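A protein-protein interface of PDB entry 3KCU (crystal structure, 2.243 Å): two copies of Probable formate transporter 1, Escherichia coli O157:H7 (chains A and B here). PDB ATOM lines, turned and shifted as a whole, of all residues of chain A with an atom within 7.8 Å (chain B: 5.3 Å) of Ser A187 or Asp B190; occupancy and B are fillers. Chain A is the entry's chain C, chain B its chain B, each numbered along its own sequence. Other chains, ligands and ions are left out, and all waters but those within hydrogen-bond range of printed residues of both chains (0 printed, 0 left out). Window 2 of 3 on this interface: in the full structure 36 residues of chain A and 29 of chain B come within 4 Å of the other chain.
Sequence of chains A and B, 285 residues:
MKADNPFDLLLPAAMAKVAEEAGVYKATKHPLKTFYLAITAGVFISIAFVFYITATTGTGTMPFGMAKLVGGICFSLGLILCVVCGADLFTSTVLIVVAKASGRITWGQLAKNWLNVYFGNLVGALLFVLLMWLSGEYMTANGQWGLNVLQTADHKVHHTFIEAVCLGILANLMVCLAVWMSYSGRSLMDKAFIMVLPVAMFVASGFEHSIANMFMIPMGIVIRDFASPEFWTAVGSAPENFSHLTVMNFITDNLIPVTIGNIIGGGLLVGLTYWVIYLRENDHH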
ATOM      1  N   VAL A  84       9.116  -4.814   4.376  1.00  0.00           N
ATOM      2  CA  VAL A  84       8.927  -3.423   4.791  1.00  0.00           C
ATOM      3  C   VAL A  84       8.700  -2.480   3.600  1.00  0.00           C
ATOM      4  O   VAL A  84       7.854  -1.581   3.674  1.00  0.00           O
ATOM      5  CB  VAL A  84      10.103  -2.921   5.677  1.00  0.00           C
ATOM      6  CG1 VAL A  84       9.948  -1.437   6.023  1.00  0.00           C
ATOM      7  CG2 VAL A  84      10.185  -3.751   6.953  1.00  0.00           C
ATOM      8  N   SER A 182       5.402 -12.565   9.767  1.00  0.00           N
ATOM      9  CA  SER A 182       5.557 -11.124   9.646  1.00  0.00           C
ATOM     10  C   SER A 182       4.208 -10.414   9.479  1.00  0.00           C
ATOM     11  O   SER A 182       3.972  -9.367  10.080  1.00  0.00           O
ATOM     12  CB  SER A 182       6.480 -10.787   8.481  1.00  0.00           C
ATOM     13  OG  SER A 182       6.665  -9.386   8.385  1.00  0.00           O
ATOM     14  N   SER A 184       1.271 -11.080  10.622  1.00  0.00           N
ATOM     15  CA  SER A 184       0.536 -10.944  11.880  1.00  0.00           C
ATOM     16  C   SER A 184       1.179  -9.876  12.770  1.00  0.00           C
ATOM     17  O   SER A 184       0.725  -9.627  13.888  1.00  0.00           O
ATOM     18  CB  SER A 184       0.499 -12.273  12.631  1.00  0.00           C
ATOM     19  OG  SER A 184       1.762 -12.541  13.224  1.00  0.00           O
ATOM     20  N   GLY A 185       2.240  -9.250  12.274  1.00  0.00           N
ATOM     21  CA  GLY A 185       2.955  -8.233  13.035  1.00  0.00           C
ATOM     22  C   GLY A 185       2.285  -6.869  13.012  1.00  0.00           C
ATOM     23  O   GLY A 185       1.666  -6.485  12.026  1.00  0.00           O
ATOM     24  N   ARG A 186       2.415  -6.120  14.095  1.00  0.00           N
ATOM     25  CA  ARG A 186       1.778  -4.809  14.155  1.00  0.00           C
ATOM     26  C   ARG A 186       2.783  -3.712  13.872  1.00  0.00           C
ATOM     27  O   ARG A 186       2.565  -2.852  13.017  1.00  0.00           O
ATOM     28  CB  ARG A 186       1.108  -4.587  15.510  1.00  0.00           C
ATOM     29  CG  ARG A 186      -0.399  -4.789  15.490  1.00  0.00           C
ATOM     30  CD  ARG A 186      -1.103  -3.616  14.816  1.00  0.00           C
ATOM     31  NE  ARG A 186      -2.558  -3.755  14.819  1.00  0.00           N
ATOM     32  CZ  ARG A 186      -3.259  -4.306  13.832  1.00  0.00           C
ATOM     33  NH1 ARG A 186      -2.638  -4.778  12.757  1.00  0.00           N
ATOM     34  NH2 ARG A 186      -4.582  -4.386  13.919  1.00  0.00           N
ATOM     35  N   SER A 187       3.903  -3.770  14.571  1.00  0.00           N
ATOM     36  CA  SER A 187       4.913  -2.739  14.474  1.00  0.00           C
ATOM     37  C   SER A 187       6.006  -3.150  13.496  1.00  0.00           C
ATOM     38  O   SER A 187       6.053  -4.298  13.037  1.00  0.00           O
ATOM     39  CB  SER A 187       5.514  -2.482  15.864  1.00  0.00           C
ATOM     40  OG  SER A 187       6.271  -3.603  16.277  1.00  0.00           O
ATOM     41  N   LEU A 188       6.878  -2.198  13.186  1.00  0.00           N
ATOM     42  CA  LEU A 188       8.047  -2.453  12.375  1.00  0.00           C
ATOM     43  C   LEU A 188       8.913  -3.546  13.011  1.00  0.00           C
ATOM     44  O   LEU A 188       9.289  -4.511  12.335  1.00  0.00           O
ATOM     45  CB  LEU A 188       8.851  -1.163  12.202  1.00  0.00           C
ATOM     46  CG  LEU A 188       9.940  -1.204  11.129  1.00  0.00           C
ATOM     47  CD1 LEU A 188       9.363  -1.831   9.866  1.00  0.00           C
ATOM     48  CD2 LEU A 188      10.494   0.183  10.850  1.00  0.00           C
ATOM     49  N   MET A 189       9.223  -3.383  14.304  1.00  0.00           N
ATOM     50  CA  MET A 189       9.948  -4.390  15.084  1.00  0.00           C
ATOM     51  C   MET A 189       9.358  -5.783  14.879  1.00  0.00           C
ATOM     52  O   MET A 189      10.088  -6.717  14.572  1.00  0.00           O
ATOM     53  CB  MET A 189       9.936  -4.059  16.586  1.00  0.00           C
ATOM     54  CG  MET A 189      10.915  -2.971  17.046  1.00  0.00           C
ATOM     55  SD  MET A 189      12.674  -3.410  16.847  1.00  0.00           S
ATOM     56  CE  MET A 189      12.987  -2.612  15.274  1.00  0.00           C
ATOM     57  N   ASP A 190       8.045  -5.915  15.088  1.00  0.00           N
ATOM     58  CA  ASP A 190       7.326  -7.169  14.848  1.00  0.00           C
ATOM     59  C   ASP A 190       7.605  -7.772  13.461  1.00  0.00           C
ATOM     60  O   ASP A 190       7.911  -8.959  13.328  1.00  0.00           O
ATOM     61  CB  ASP A 190       5.812  -6.938  14.933  1.00  0.00           C
ATOM     62  CG  ASP A 190       5.308  -6.776  16.354  1.00  0.00           C
ATOM     63  OD1 ASP A 190       6.058  -7.047  17.321  1.00  0.00           O
ATOM     64  OD2 ASP A 190       4.129  -6.386  16.498  1.00  0.00           O
ATOM     65  N   LYS A 191       7.460  -6.953  12.426  1.00  0.00           N
ATOM     66  CA  LYS A 191       7.468  -7.472  11.061  1.00  0.00           C
ATOM     67  C   LYS A 191       8.872  -7.842  10.597  1.00  0.00           C
ATOM     68  O   LYS A 191       9.047  -8.793   9.827  1.00  0.00           O
ATOM     69  CB  LYS A 191       6.833  -6.474  10.083  1.00  0.00           C
ATOM     70  CG  LYS A 191       5.405  -6.072  10.429  1.00  0.00           C
ATOM     71  CD  LYS A 191       4.845  -5.071   9.430  1.00  0.00           C
ATOM     72  CE  LYS A 191       3.417  -4.700   9.786  1.00  0.00           C
ATOM     73  NZ  LYS A 191       2.868  -3.708   8.835  1.00  0.00           N
ATOM     74  N   ALA A 192       9.864  -7.084  11.057  1.00  0.00           N
ATOM     75  CA  ALA A 192      11.245  -7.337  10.664  1.00  0.00           C
ATOM     76  C   ALA A 192      11.796  -8.525  11.431  1.00  0.00           C
ATOM     77  O   ALA A 192      12.231  -9.520  10.842  1.00  0.00           O
ATOM     78  CB  ALA A 192      12.117  -6.105  10.902  1.00  0.00           C
ATOM     79  N   PHE A 193      11.745  -8.432  12.755  1.00  0.00           N
ATOM     80  CA  PHE A 193      12.551  -9.316  13.584  1.00  0.00           C
ATOM     81  C   PHE A 193      11.967 -10.706  13.835  1.00  0.00           C
ATOM     82  O   PHE A 193      12.681 -11.625  14.259  1.00  0.00           O
ATOM     83  CB  PHE A 193      13.008  -8.589  14.846  1.00  0.00           C
ATOM     84  CG  PHE A 193      13.932  -7.432  14.550  1.00  0.00           C
ATOM     85  CD1 PHE A 193      15.249  -7.660  14.164  1.00  0.00           C
ATOM     86  CD2 PHE A 193      13.482  -6.120  14.615  1.00  0.00           C
ATOM     87  CE1 PHE A 193      16.102  -6.603  13.872  1.00  0.00           C
ATOM     88  CE2 PHE A 193      14.336  -5.063  14.322  1.00  0.00           C
ATOM     89  CZ  PHE A 193      15.642  -5.303  13.949  1.00  0.00           C
ATOM     90  N   SER B 182      13.085   3.335   8.367  1.00  0.00           N
ATOM     91  CA  SER B 182      12.953   4.028   9.640  1.00  0.00           C
ATOM     92  C   SER B 182      11.667   4.875   9.653  1.00  0.00           C
ATOM     93  O   SER B 182      10.985   4.988  10.680  1.00  0.00           O
ATOM     94  CB  SER B 182      14.203   4.884   9.893  1.00  0.00           C
ATOM     95  OG  SER B 182      14.141   5.566  11.124  1.00  0.00           O
ATOM     96  N   GLY B 185       8.357   3.447  10.810  1.00  0.00           N
ATOM     97  CA  GLY B 185       8.340   3.039  12.203  1.00  0.00           C
ATOM     98  C   GLY B 185       7.496   3.953  13.080  1.00  0.00           C
ATOM     99  O   GLY B 185       7.302   5.130  12.777  1.00  0.00           O
ATOM    100  N   ARG B 186       6.998   3.424  14.185  1.00  0.00           N
ATOM    101  CA  ARG B 186       6.171   4.231  15.064  1.00  0.00           C
ATOM    102  C   ARG B 186       6.833   4.420  16.432  1.00  0.00           C
ATOM    103  O   ARG B 186       6.850   5.527  16.970  1.00  0.00           O
ATOM    104  CB  ARG B 186       4.765   3.633  15.155  1.00  0.00           C
ATOM    105  CG  ARG B 186       4.189   3.320  13.764  1.00  0.00           C
ATOM    106  CD  ARG B 186       2.740   2.855  13.793  1.00  0.00           C
ATOM    107  NE  ARG B 186       1.798   3.955  13.598  1.00  0.00           N
ATOM    108  CZ  ARG B 186       0.942   4.383  14.524  1.00  0.00           C
ATOM    109  NH1 ARG B 186       0.903   3.802  15.717  1.00  0.00           N
ATOM    110  NH2 ARG B 186       0.121   5.391  14.255  1.00  0.00           N
ATOM    111  N   SER B 187       7.413   3.355  16.974  1.00  0.00           N
ATOM    112  CA  SER B 187       8.164   3.458  18.221  1.00  0.00           C
ATOM    113  C   SER B 187       9.622   3.829  17.959  1.00  0.00           C
ATOM    114  O   SER B 187      10.104   3.807  16.818  1.00  0.00           O
ATOM    115  CB  SER B 187       8.099   2.143  19.007  1.00  0.00           C
ATOM    116  OG  SER B 187       8.831   1.106  18.357  1.00  0.00           O
ATOM    117  N   LEU B 188      10.317   4.169  19.034  1.00  0.00           N
ATOM    118  CA  LEU B 188      11.721   4.496  18.970  1.00  0.00           C
ATOM    119  C   LEU B 188      12.560   3.258  18.609  1.00  0.00           C
ATOM    120  O   LEU B 188      13.483   3.350  17.804  1.00  0.00           O
ATOM    121  CB  LEU B 188      12.147   5.091  20.300  1.00  0.00           C
ATOM    122  CG  LEU B 188      13.567   5.609  20.429  1.00  0.00           C
ATOM    123  CD1 LEU B 188      13.918   6.437  19.218  1.00  0.00           C
ATOM    124  CD2 LEU B 188      13.701   6.420  21.743  1.00  0.00           C
ATOM    125  N   MET B 189      12.225   2.106  19.192  1.00  0.00           N
ATOM    126  CA  MET B 189      12.826   0.828  18.788  1.00  0.00           C
ATOM    127  C   MET B 189      12.722   0.607  17.271  1.00  0.00           C
ATOM    128  O   MET B 189      13.721   0.277  16.615  1.00  0.00           O
ATOM    129  CB  MET B 189      12.168  -0.340  19.533  1.00  0.00           C
ATOM    130  CG  MET B 189      12.462  -0.370  21.031  1.00  0.00           C
ATOM    131  SD  MET B 189      14.176  -0.849  21.367  1.00  0.00           S
ATOM    132  CE  MET B 189      14.159  -2.527  20.720  1.00  0.00           C
ATOM    133  N   ASP B 190      11.511   0.775  16.734  1.00  0.00           N
ATOM    134  CA  ASP B 190      11.269   0.648  15.292  1.00  0.00           C
ATOM    135  C   ASP B 190      12.261   1.477  14.506  1.00  0.00           C
ATOM    136  O   ASP B 190      13.007   0.957  13.692  1.00  0.00           O
ATOM    137  CB  ASP B 190       9.880   1.163  14.911  1.00  0.00           C
ATOM    138  CG  ASP B 190       8.757   0.215  15.288  1.00  0.00           C
ATOM    139  OD1 ASP B 190       9.004  -0.969  15.599  1.00  0.00           O
ATOM    140  OD2 ASP B 190       7.602   0.678  15.263  1.00  0.00           O
ATOM    141  N   LYS B 191      12.255   2.780  14.771  1.00  0.00           N
ATOM    142  CA  LYS B 191      12.952   3.743  13.935  1.00  0.00           C
ATOM    143  C   LYS B 191      14.465   3.567  14.001  1.00  0.00           C
ATOM    144  O   LYS B 191      15.162   3.763  13.000  1.00  0.00           O
ATOM    145  CB  LYS B 191      12.568   5.174  14.339  1.00  0.00           C
ATOM    146  CG  LYS B 191      11.120   5.592  14.013  1.00  0.00           C
ATOM    147  CD  LYS B 191      10.823   6.975  14.632  1.00  0.00           C
ATOM    148  CE  LYS B 191       9.406   7.489  14.307  1.00  0.00           C
ATOM    149  NZ  LYS B 191       9.161   8.786  14.991  1.00  0.00           N
ATOM    150  N   ALA B 192      14.964   3.195  15.180  1.00  0.00           N
ATOM    151  CA  ALA B 192      16.401   2.999  15.389  1.00  0.00           C
ATOM    152  C   ALA B 192      16.871   1.636  14.915  1.00  0.00           C
ATOM    153  O   ALA B 192      17.781   1.535  14.091  1.00  0.00           O
ATOM    154  CB  ALA B 192      16.762   3.185  16.857  1.00  0.00           C
ATOM    155  N   PHE B 193      16.245   0.582  15.426  1.00  0.00           N
ATOM    156  CA  PHE B 193      16.777  -0.760  15.181  1.00  0.00           C
ATOM    157  C   PHE B 193      16.560  -1.300  13.772  1.00  0.00           C
ATOM    158  O   PHE B 193      17.279  -2.196  13.332  1.00  0.00           O
ATOM    159  CB  PHE B 193      16.327  -1.744  16.271  1.00  0.00           C
ATOM    160  CG  PHE B 193      17.004  -1.494  17.594  1.00  0.00           C
ATOM    161  CD1 PHE B 193      18.179  -2.166  17.928  1.00  0.00           C
ATOM    162  CD2 PHE B 193      16.509  -0.544  18.475  1.00  0.00           C
ATOM    163  CE1 PHE B 193      18.827  -1.919  19.136  1.00  0.00           C
ATOM    164  CE2 PHE B 193      17.155  -0.289  19.690  1.00  0.00           C
ATOM    165  CZ  PHE B 193      18.311  -0.976  20.018  1.00  0.00           C
ATOM    166  N   ILE B 194      15.586  -0.749  13.055  1.00  0.00           N
ATOM    167  CA  ILE B 194      15.347  -1.215  11.696  1.00  0.00           C
ATOM    168  C   ILE B 194      16.548  -0.810  10.854  1.00  0.00           C
ATOM    169  O   ILE B 194      16.775  -1.356   9.786  1.00  0.00           O
ATOM    170  CB  ILE B 194      14.031  -0.623  11.089  1.00  0.00           C
ATOM    171  CG1 ILE B 194      13.615  -1.397   9.829  1.00  0.00           C
ATOM    172  CG2 ILE B 194      14.199   0.866  10.792  1.00  0.00           C
ATOM    173  CD1 ILE B 194      13.372  -2.855  10.089  1.00  0.00           C
ATOM    174  N   MET B 195      17.332   0.149  11.345  1.00  0.00           N
ATOM    175  CA  MET B 195      18.447   0.660  10.557  1.00  0.00           C
ATOM    176  C   MET B 195      19.764  -0.067  10.816  1.00  0.00           C
ATOM    177  O   MET B 195      20.711   0.126  10.077  1.00  0.00           O
ATOM    178  CB  MET B 195      18.642   2.164  10.761  1.00  0.00           C
ATOM    179  CG  MET B 195      17.484   3.035  10.206  1.00  0.00           C
ATOM    180  SD  MET B 195      17.884   4.797  10.174  1.00  0.00           S
ATOM    181  CE  MET B 195      18.107   5.175  11.903  1.00  0.00           C
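OD1 of Asp B190 is in hydrogen-bond range of N of Met A189, at 2.7 Å. OD1 of Asp B190 sits close to N of Leu A188.
The side-chain hydroxyl of Ser A187 is in hydrogen-bond range of the backbone NH of Asp A190 (3.1 Å). N of Asp B190 sits at hydrogen-bond distance from OG of Ser B187 (3.2 Å). N of Arg B186 sits at hydrogen-bond distance from OD2 of Asp B190 (3.0 Å).
Among the printed residues, merely in contact across the chains: Ser A187 with Asp B190 (3.8 Å), Leu A188 with Gly B185 (3.8 Å), Leu A188 with Ile B194 (3.6 Å), Met A189 with Met B189 (3.3 Å), Met A189 with Phe B193 (3.6 Å), Met A189 with Ile B194 (3.9 Å), Ala A192 with Ile B194 (3.6 Å) and Phe A193 with Phe B193 (3.6 Å).
Printed residues of chain B within 4 Å of Ser A187: Asp B190 (3.8 Å). Of the printed residues of chain A, Asp B190 touches Ser A187, Leu A188 and Met A189. Printed residues of chain A within 4 Å of Gly B185: Leu A188. Printed residues of chain B within 4 Å of Ala A192: Ile B194 (3.6 Å). Printed residues of chain A within 4 Å of Ile B194: Leu A188 (3.6 Å), Met A189 (3.9 Å) and Ala A192 (3.6 Å). The nearest residue of chain A that does not touch Asp B190 is Asp A190 (5.1 Å). The nearest printed residue of chain B that does not touch Leu A188 is Ser B182 (4.7 Å).
Along chain B the printed residues that touch a printed residue of chain A span positions 185 to 194. Hydrophobic or aromatic side chains of chain A within 4 Å of the printed part of chain B: Leu A188, Met A189, Ala A192 and Phe A193. Among the printed residues, 10 pairs touch across the chains.
Ser A187 touches Asp B190, but with the chains exchanged Asp A190 does not touch Ser B187 (7.8 Å). Leu A188 touches Gly B185, but with the chains exchanged Gly A185 does not touch Leu B188 (14.9 Å). Met A189 touches Phe B193, but with the chains exchanged Phe A193 does not touch Met B189 (5.8 Å). Phe A193 touches its own counterpart, Phe B193. 10 positions are printed for both chains. Of the 10 pairs that touch across the chains among the printed residues, 2 have their exchanged pair printed and touching as well.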
